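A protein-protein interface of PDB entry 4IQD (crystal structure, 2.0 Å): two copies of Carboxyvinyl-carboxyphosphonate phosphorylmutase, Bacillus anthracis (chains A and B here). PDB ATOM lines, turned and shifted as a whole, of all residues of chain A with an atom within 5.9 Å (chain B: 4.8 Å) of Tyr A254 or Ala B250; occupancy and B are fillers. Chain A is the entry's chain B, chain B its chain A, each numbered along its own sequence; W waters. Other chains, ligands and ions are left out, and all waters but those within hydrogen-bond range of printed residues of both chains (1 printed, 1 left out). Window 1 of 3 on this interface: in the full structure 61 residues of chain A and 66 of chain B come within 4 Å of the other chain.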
ATOM      1  N   HIS A  37      10.640 -11.813  38.519  1.00  0.00           N
ATOM      2  CA  HIS A  37      11.423 -10.761  39.156  1.00  0.00           C
ATOM      3  C   HIS A  37      10.570  -9.821  40.005  1.00  0.00           C
ATOM      4  O   HIS A  37      11.086  -9.131  40.879  1.00  0.00           O
ATOM      5  CB  HIS A  37      12.223  -9.972  38.121  1.00  0.00           C
ATOM      6  CG  HIS A  37      11.375  -9.270  37.114  1.00  0.00           C
ATOM      7  ND1 HIS A  37      10.776  -9.926  36.061  1.00  0.00           N
ATOM      8  CD2 HIS A  37      11.022  -7.967  36.996  1.00  0.00           C
ATOM      9  CE1 HIS A  37      10.093  -9.059  35.337  1.00  0.00           C
ATOM     10  NE2 HIS A  37      10.225  -7.865  35.882  1.00  0.00           N
ATOM     11  N   LEU A 247      12.414 -10.896  32.785  1.00  0.00           N
ATOM     12  CA  LEU A 247      13.045  -9.603  32.585  1.00  0.00           C
ATOM     13  C   LEU A 247      13.518  -9.426  31.148  1.00  0.00           C
ATOM     14  O   LEU A 247      13.472  -8.322  30.601  1.00  0.00           O
ATOM     15  CB  LEU A 247      14.216  -9.408  33.539  1.00  0.00           C
ATOM     16  CG  LEU A 247      14.752  -7.984  33.419  1.00  0.00           C
ATOM     17  CD1 LEU A 247      13.904  -7.005  34.217  1.00  0.00           C
ATOM     18  CD2 LEU A 247      16.205  -7.907  33.811  1.00  0.00           C
ATOM     19  N   VAL A 249      12.128 -10.498  28.437  1.00  0.00           N
ATOM     20  CA  VAL A 249      11.009 -10.100  27.589  1.00  0.00           C
ATOM     21  C   VAL A 249      10.434  -8.756  28.011  1.00  0.00           C
ATOM     22  O   VAL A 249       9.882  -8.028  27.191  1.00  0.00           O
ATOM     23  CB  VAL A 249       9.875 -11.157  27.550  1.00  0.00           C
ATOM     24  CG1 VAL A 249      10.364 -12.455  26.924  1.00  0.00           C
ATOM     25  CG2 VAL A 249       9.304 -11.396  28.933  1.00  0.00           C
ATOM     26  N   ALA A 250      10.563  -8.426  29.291  1.00  0.00           N
ATOM     27  CA  ALA A 250      10.038  -7.163  29.788  1.00  0.00           C
ATOM     28  C   ALA A 250      10.834  -6.004  29.210  1.00  0.00           C
ATOM     29  O   ALA A 250      10.270  -5.006  28.764  1.00  0.00           O
ATOM     30  CB  ALA A 250      10.076  -7.130  31.305  1.00  0.00           C
ATOM     31  N   ALA A 251      12.151  -6.156  29.213  1.00  0.00           N
ATOM     32  CA  ALA A 251      13.050  -5.125  28.726  1.00  0.00           C
ATOM     33  C   ALA A 251      12.764  -4.769  27.271  1.00  0.00           C
ATOM     34  O   ALA A 251      12.574  -3.603  26.936  1.00  0.00           O
ATOM     35  CB  ALA A 251      14.477  -5.588  28.878  1.00  0.00           C
ATOM     36  N   LYS A 252      12.725  -5.784  26.414  1.00  0.00           N
ATOM     37  CA  LYS A 252      12.572  -5.580  24.976  1.00  0.00           C
ATOM     38  C   LYS A 252      11.241  -4.915  24.648  1.00  0.00           C
ATOM     39  O   LYS A 252      11.146  -4.128  23.706  1.00  0.00           O
ATOM     40  CB  LYS A 252      12.701  -6.912  24.229  1.00  0.00           C
ATOM     41  CG  LYS A 252      13.525  -6.843  22.945  1.00  0.00           C
ATOM     42  CD  LYS A 252      12.757  -6.185  21.820  1.00  0.00           C
ATOM     43  CE  LYS A 252      13.454  -6.372  20.479  1.00  0.00           C
ATOM     44  NZ  LYS A 252      14.766  -5.676  20.417  1.00  0.00           N
ATOM     45  N   ALA A 253      10.219  -5.232  25.437  1.00  0.00           N
ATOM     46  CA  ALA A 253       8.904  -4.624  25.272  1.00  0.00           C
ATOM     47  C   ALA A 253       8.941  -3.136  25.602  1.00  0.00           C
ATOM     48  O   ALA A 253       8.282  -2.334  24.940  1.00  0.00           O
ATOM     49  CB  ALA A 253       7.877  -5.335  26.134  1.00  0.00           C
ATOM     50  N   TYR A 254       9.697  -2.774  26.634  1.00  0.00           N
ATOM     51  CA  TYR A 254       9.893  -1.370  26.967  1.00  0.00           C
ATOM     52  C   TYR A 254      10.500  -0.688  25.757  1.00  0.00           C
ATOM     53  O   TYR A 254      10.003   0.334  25.291  1.00  0.00           O
ATOM     54  CB  TYR A 254      10.854  -1.204  28.146  1.00  0.00           C
ATOM     55  CG  TYR A 254      10.425  -1.847  29.444  1.00  0.00           C
ATOM     56  CD1 TYR A 254       9.088  -2.094  29.720  1.00  0.00           C
ATOM     57  CD2 TYR A 254      11.369  -2.200  30.402  1.00  0.00           C
ATOM     58  CE1 TYR A 254       8.704  -2.682  30.909  1.00  0.00           C
ATOM     59  CE2 TYR A 254      10.995  -2.785  31.592  1.00  0.00           C
ATOM     60  CZ  TYR A 254       9.662  -3.024  31.841  1.00  0.00           C
ATOM     61  OH  TYR A 254       9.287  -3.609  33.026  1.00  0.00           O
ATOM     62  N   GLU A 255      11.577  -1.284  25.253  1.00  0.00           N
ATOM     63  CA  GLU A 255      12.343  -0.735  24.143  1.00  0.00           C
ATOM     64  C   GLU A 255      11.458  -0.439  22.954  1.00  0.00           C
ATOM     65  O   GLU A 255      11.522   0.644  22.379  1.00  0.00           O
ATOM     66  CB  GLU A 255      13.444  -1.713  23.725  1.00  0.00           C
ATOM     67  CG  GLU A 255      14.287  -1.244  22.547  1.00  0.00           C
ATOM     68  CD  GLU A 255      15.317  -2.277  22.116  1.00  0.00           C
ATOM     69  OE1 GLU A 255      15.051  -3.489  22.259  1.00  0.00           O
ATOM     70  OE2 GLU A 255      16.398  -1.874  21.635  1.00  0.00           O
ATOM     71  N   ASN A 256      10.627  -1.409  22.594  1.00  0.00           N
ATOM     72  CA  ASN A 256       9.776  -1.281  21.423  1.00  0.00           C
ATOM     73  C   ASN A 256       8.680  -0.240  21.581  1.00  0.00           C
ATOM     74  O   ASN A 256       8.404   0.522  20.659  1.00  0.00           O
ATOM     75  CB  ASN A 256       9.178  -2.635  21.037  1.00  0.00           C
ATOM     76  CG  ASN A 256      10.214  -3.586  20.464  1.00  0.00           C
ATOM     77  OD1 ASN A 256      11.272  -3.165  19.995  1.00  0.00           O
ATOM     78  ND2 ASN A 256       9.908  -4.878  20.497  1.00  0.00           N
ATOM     79  N   VAL A 257       8.055  -0.200  22.750  1.00  0.00           N
ATOM     80  CA  VAL A 257       6.971   0.743  22.948  1.00  0.00           C
ATOM     81  C   VAL A 257       7.506   2.158  23.164  1.00  0.00           C
ATOM     82  O   VAL A 257       6.911   3.124  22.694  1.00  0.00           O
ATOM     83  CB  VAL A 257       6.009   0.310  24.081  1.00  0.00           C
ATOM     84  CG1 VAL A 257       6.655   0.464  25.450  1.00  0.00           C
ATOM     85  CG2 VAL A 257       4.713   1.095  24.001  1.00  0.00           C
ATOM     86  N   PHE A 258       8.641   2.276  23.845  1.00  0.00           N
ATOM     87  CA  PHE A 258       9.231   3.585  24.098  1.00  0.00           C
ATOM     88  C   PHE A 258       9.735   4.223  22.813  1.00  0.00           C
ATOM     89  O   PHE A 258       9.597   5.429  22.612  1.00  0.00           O
ATOM     90  CB  PHE A 258      10.369   3.478  25.110  1.00  0.00           C
ATOM     91  CG  PHE A 258       9.901   3.318  26.523  1.00  0.00           C
ATOM     92  CD1 PHE A 258       8.771   3.981  26.968  1.00  0.00           C
ATOM     93  CD2 PHE A 258      10.587   2.504  27.405  1.00  0.00           C
ATOM     94  CE1 PHE A 258       8.337   3.834  28.270  1.00  0.00           C
ATOM     95  CE2 PHE A 258      10.156   2.352  28.707  1.00  0.00           C
ATOM     96  CZ  PHE A 258       9.029   3.020  29.141  1.00  0.00           C
ATOM     97  N   THR A 259      10.329   3.405  21.954  1.00  0.00           N
ATOM     98  CA  THR A 259      10.803   3.870  20.664  1.00  0.00           C
ATOM     99  C   THR A 259       9.609   4.325  19.852  1.00  0.00           C
ATOM    100  O   THR A 259       9.647   5.363  19.190  1.00  0.00           O
ATOM    101  CB  THR A 259      11.534   2.747  19.909  1.00  0.00           C
ATOM    102  OG1 THR A 259      12.703   2.363  20.641  1.00  0.00           O
ATOM    103  CG2 THR A 259      11.944   3.209  18.532  1.00  0.00           C
ATOM    104  N   ASN A 273      -0.263  -5.117  21.883  1.00  0.00           N
ATOM    105  CA  ASN A 273       0.859  -5.670  22.641  1.00  0.00           C
ATOM    106  C   ASN A 273       0.772  -5.349  24.125  1.00  0.00           C
ATOM    107  O   ASN A 273       1.791  -5.275  24.809  1.00  0.00           O
ATOM    108  CB  ASN A 273       2.198  -5.167  22.086  1.00  0.00           C
ATOM    109  CG  ASN A 273       2.546  -5.781  20.742  1.00  0.00           C
ATOM    110  OD1 ASN A 273       1.986  -5.409  19.715  1.00  0.00           O
ATOM    111  ND2 ASN A 273       3.485  -6.719  20.744  1.00  0.00           N
ATOM    112  N   HIS B  37       7.756   1.975  36.028  1.00  0.00           N
ATOM    113  CA  HIS B  37       7.380   1.340  37.287  1.00  0.00           C
ATOM    114  C   HIS B  37       8.571   0.748  38.029  1.00  0.00           C
ATOM    115  O   HIS B  37       8.467   0.426  39.211  1.00  0.00           O
ATOM    116  CB  HIS B  37       6.313   0.270  37.062  1.00  0.00           C
ATOM    117  CG  HIS B  37       6.764  -0.864  36.190  1.00  0.00           C
ATOM    118  ND1 HIS B  37       6.754  -0.792  34.820  1.00  0.00           N
ATOM    119  CD2 HIS B  37       7.227  -2.094  36.504  1.00  0.00           C
ATOM    120  CE1 HIS B  37       7.199  -1.931  34.314  1.00  0.00           C
ATOM    121  NE2 HIS B  37       7.491  -2.741  35.326  1.00  0.00           N
ATOM    122  N   ASP B  38       9.698   0.602  37.334  1.00  0.00           N
ATOM    123  CA  ASP B  38      10.914   0.090  37.955  1.00  0.00           C
ATOM    124  C   ASP B  38      12.179   0.651  37.301  1.00  0.00           C
ATOM    125  O   ASP B  38      12.106   1.355  36.293  1.00  0.00           O
ATOM    126  CB  ASP B  38      10.921  -1.445  37.962  1.00  0.00           C
ATOM    127  CG  ASP B  38      11.199  -2.050  36.591  1.00  0.00           C
ATOM    128  OD1 ASP B  38      11.194  -1.322  35.578  1.00  0.00           O
ATOM    129  OD2 ASP B  38      11.413  -3.278  36.527  1.00  0.00           O
ATOM    130  N   MET B  40      14.618  -0.778  35.615  1.00  0.00           N
ATOM    131  CA  MET B  40      14.934  -1.245  34.265  1.00  0.00           C
ATOM    132  C   MET B  40      14.155  -0.466  33.213  1.00  0.00           C
ATOM    133  O   MET B  40      14.718  -0.053  32.202  1.00  0.00           O
ATOM    134  CB  MET B  40      14.693  -2.748  34.105  1.00  0.00           C
ATOM    135  CG  MET B  40      14.988  -3.266  32.697  1.00  0.00           C
ATOM    136  SD  MET B  40      16.822  -2.912  32.119  1.00  0.00           S
ATOM    137  CE  MET B  40      16.648  -3.281  30.225  1.00  0.00           C
ATOM    138  N   ALA B  41      12.862  -0.267  33.455  1.00  0.00           N
ATOM    139  CA  ALA B  41      12.041   0.545  32.567  1.00  0.00           C
ATOM    140  C   ALA B  41      12.588   1.968  32.500  1.00  0.00           C
ATOM    141  O   ALA B  41      12.580   2.596  31.444  1.00  0.00           O
ATOM    142  CB  ALA B  41      10.588   0.548  33.029  1.00  0.00           C
ATOM    143  N   VAL B  44      15.644   2.002  30.158  1.00  0.00           N
ATOM    144  CA  VAL B  44      15.270   1.871  28.754  1.00  0.00           C
ATOM    145  C   VAL B  44      14.705   3.177  28.210  1.00  0.00           C
ATOM    146  O   VAL B  44      14.981   3.557  27.073  1.00  0.00           O
ATOM    147  CB  VAL B  44      14.235   0.759  28.543  1.00  0.00           C
ATOM    148  CG1 VAL B  44      13.910   0.621  27.072  1.00  0.00           C
ATOM    149  CG2 VAL B  44      14.754  -0.546  29.083  1.00  0.00           C
ATOM    150  N   SER B 246       4.407   1.010  30.429  1.00  0.00           N
ATOM    151  CA  SER B 246       5.534   0.121  30.702  1.00  0.00           C
ATOM    152  C   SER B 246       5.089  -1.205  31.312  1.00  0.00           C
ATOM    153  O   SER B 246       5.609  -2.260  30.962  1.00  0.00           O
ATOM    154  CB  SER B 246       6.553   0.803  31.619  1.00  0.00           C
ATOM    155  OG  SER B 246       6.016   1.013  32.911  1.00  0.00           O
ATOM    156  N   LEU B 247       4.118  -1.149  32.215  1.00  0.00           N
ATOM    157  CA  LEU B 247       3.630  -2.349  32.883  1.00  0.00           C
ATOM    158  C   LEU B 247       2.655  -3.127  32.005  1.00  0.00           C
ATOM    159  O   LEU B 247       2.599  -4.356  32.067  1.00  0.00           O
ATOM    160  CB  LEU B 247       2.986  -1.995  34.226  1.00  0.00           C
ATOM    161  CG  LEU B 247       2.361  -3.153  35.008  1.00  0.00           C
ATOM    162  CD1 LEU B 247       2.807  -3.130  36.459  1.00  0.00           C
ATOM    163  CD2 LEU B 247       0.844  -3.096  34.914  1.00  0.00           C
ATOM    164  N   ARG B 248       1.892  -2.409  31.187  1.00  0.00           N
ATOM    165  CA  ARG B 248       0.928  -3.039  30.294  1.00  0.00           C
ATOM    166  C   ARG B 248       1.608  -3.960  29.295  1.00  0.00           C
ATOM    167  O   ARG B 248       1.157  -5.080  29.070  1.00  0.00           O
ATOM    168  CB  ARG B 248       0.115  -1.991  29.541  1.00  0.00           C
ATOM    169  CG  ARG B 248      -0.770  -1.132  30.416  1.00  0.00           C
ATOM    170  CD  ARG B 248      -2.024  -0.753  29.659  1.00  0.00           C
ATOM    171  NE  ARG B 248      -2.643   0.469  30.156  1.00  0.00           N
ATOM    172  CZ  ARG B 248      -3.533   0.510  31.140  1.00  0.00           C
ATOM    173  NH1 ARG B 248      -3.897  -0.611  31.750  1.00  0.00           N
ATOM    174  NH2 ARG B 248      -4.051   1.672  31.519  1.00  0.00           N
ATOM    175  N   VAL B 249       2.692  -3.477  28.695  1.00  0.00           N
ATOM    176  CA  VAL B 249       3.432  -4.249  27.704  1.00  0.00           C
ATOM    177  C   VAL B 249       4.238  -5.374  28.349  1.00  0.00           C
ATOM    178  O   VAL B 249       4.412  -6.441  27.759  1.00  0.00           O
ATOM    179  CB  VAL B 249       4.371  -3.350  26.862  1.00  0.00           C
ATOM    180  CG1 VAL B 249       3.568  -2.404  25.989  1.00  0.00           C
ATOM    181  CG2 VAL B 249       5.317  -2.572  27.755  1.00  0.00           C
ATOM    182  N   ALA B 250       4.722  -5.134  29.563  1.00  0.00           N
ATOM    183  CA  ALA B 250       5.516  -6.120  30.278  1.00  0.00           C
ATOM    184  C   ALA B 250       4.645  -7.293  30.693  1.00  0.00           C
ATOM    185  O   ALA B 250       5.039  -8.451  30.559  1.00  0.00           O
ATOM    186  CB  ALA B 250       6.172  -5.490  31.494  1.00  0.00           C
ATOM    187  N   ALA B 251       3.455  -6.984  31.195  1.00  0.00           N
ATOM    188  CA  ALA B 251       2.529  -8.012  31.647  1.00  0.00           C
ATOM    189  C   ALA B 251       2.072  -8.868  30.473  1.00  0.00           C
ATOM    190  O   ALA B 251       1.853 -10.067  30.616  1.00  0.00           O
ATOM    191  CB  ALA B 251       1.345  -7.384  32.349  1.00  0.00           C
ATOM    192  N   LYS B 252       1.944  -8.243  29.308  1.00  0.00           N
ATOM    193  CA  LYS B 252       1.591  -8.962  28.094  1.00  0.00           C
ATOM    194  C   LYS B 252       2.709  -9.924  27.713  1.00  0.00           C
ATOM    195  O   LYS B 252       2.457 -11.053  27.287  1.00  0.00           O
ATOM    196  CB  LYS B 252       1.345  -7.978  26.951  1.00  0.00           C
ATOM    197  CG  LYS B 252       0.693  -8.604  25.737  1.00  0.00           C
ATOM    198  CD  LYS B 252      -0.619  -9.262  26.112  1.00  0.00           C
ATOM    199  CE  LYS B 252      -1.341  -9.804  24.893  1.00  0.00           C
ATOM    200  NZ  LYS B 252      -2.629 -10.458  25.255  1.00  0.00           N
ATOM    201  N   ALA B 253       3.945  -9.468  27.882  1.00  0.00           N
ATOM    202  CA  ALA B 253       5.118 -10.245  27.504  1.00  0.00           C
ATOM    203  C   ALA B 253       5.325 -11.454  28.410  1.00  0.00           C
ATOM    204  O   ALA B 253       5.776 -12.500  27.952  1.00  0.00           O
ATOM    205  CB  ALA B 253       6.359  -9.365  27.494  1.00  0.00           C
ATOM    206  N   TYR B 254       4.998 -11.310  29.691  1.00  0.00           N
ATOM    207  CA  TYR B 254       5.066 -12.438  30.610  1.00  0.00           C
ATOM    208  C   TYR B 254       4.130 -13.521  30.096  1.00  0.00           C
ATOM    209  O   TYR B 254       4.527 -14.672  29.915  1.00  0.00           O
ATOM    210  CB  TYR B 254       4.630 -12.029  32.017  1.00  0.00           C
ATOM    211  CG  TYR B 254       5.436 -10.913  32.639  1.00  0.00           C
ATOM    212  CD1 TYR B 254       6.770 -10.720  32.310  1.00  0.00           C
ATOM    213  CD2 TYR B 254       4.856 -10.054  33.561  1.00  0.00           C
ATOM    214  CE1 TYR B 254       7.503  -9.699  32.881  1.00  0.00           C
ATOM    215  CE2 TYR B 254       5.579  -9.037  34.138  1.00  0.00           C
ATOM    216  CZ  TYR B 254       6.901  -8.860  33.795  1.00  0.00           C
ATOM    217  OH  TYR B 254       7.621  -7.840  34.371  1.00  0.00           O
HETATM  218  O   HOH W   1       4.058  -6.753  25.330  1.00  0.00           O
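His A37 touches Tyr B254, and with the chains exchanged Tyr A254 touches His B37.
Val A249 touches Ala B253, and with the chains exchanged Ala A253 touches Val B249.
Ala A250 touches Tyr B254, and with the chains exchanged Tyr A254 touches Ala B250.
Positions printed for both chains: 37, 247, 249, 250, 251, 252, 253 and 254.
Of chain B, only His B37 (3.0 Å), Asp B38 (3.9 Å), Ala B41 (3.6 Å), Val B44 (3.7 Å), Ser B246 (3.1 Å) and Ala B250 (3.8 Å) come within 4 Å of Tyr A254.
Ala B250 touches just one residue of chain A: Tyr A254 (3.8 Å).
Of the printed residues of chain A, Lys B252 touches Asn A273 (3.5 Å).
Printed residues of chain B within 4 Å of Val A249: Ala B253 (3.8 Å).
Printed residues of chain A within 4 Å of Ser B246: Tyr A254.
Of the printed residues of chain B, Phe A258 touches Ala B41 (3.7 Å) and Val B44 (3.8 Å).
Thr A259 touches none of the printed residues of chain B.
The nearest residue of chain B that does not touch Tyr A254 is Met B40 (4.2 Å).
The nearest residue of chain A that does not touch Ala B250 is Ala A250 (4.2 Å).
The nearest printed residue of chain A that does not touch Met B40 is Tyr A254 (4.2 Å).
Water W1 lies within hydrogen-bond range of the backbone carbonyl oxygen of Val B249 (2.5 Å) and the backbone carbonyl oxygen of Asn A273 (2.8 Å).
Hydrophobic or aromatic side chains of chain A within 4 Å of the printed part of chain B: His A37, Val A249, Ala A250, Ala A251, Ala A253, Tyr A254 and Phe A258.
Among the printed residues, merely in contact across the chains: Val A249 with Ala B253 (3.8 Å), Ala A250 with Tyr B254 (3.96 Å), Ala A251 with Met B40 (3.4 Å), Ala A253 with Val B249 (3.98 Å), Tyr A254 with Asp B38 (3.9 Å), Tyr A254 with Ala B41 (3.6 Å), Tyr A254 with Val B44 (3.7 Å), Tyr A254 with Ser B246 (3.1 Å), Tyr A254 with Ala B250 (3.8 Å), Glu A255 with Val B44 (3.5 Å), Phe A258 with Ala B41 (3.7 Å), Phe A258 with Val B44 (3.8 Å), Asn A273 with Val B249 (3.5 Å) and Asn A273 with Lys B252 (3.5 Å).
ND1 of His B37 is in hydrogen-bond range of OG of Ser B246, at 2.7 Å.
The side-chain carboxylate (OD1) of Asp B38 lies close to the backbone NH (N) of Met B40.
The side-chain carboxylate (OD1) of Asp B38 sits at hydrogen-bond distance from the backbone NH (N) of Ala B41 (2.9 Å).
The side-chain amino group (NZ) of Lys A252 lies within salt-bridge range of the side-chain carboxylate (OE1) of Glu A255, 2.9 Å away.
O of Glu A255 lies within hydrogen-bond range of OG1 of Thr A259 (2.7 Å).
NE2 of His B37 sits close to OH of Tyr A254 (3.0 Å).
The side-chain hydroxyl of Tyr B254 sits close to a ring nitrogen (NE2) of His A37 (3.0 Å).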
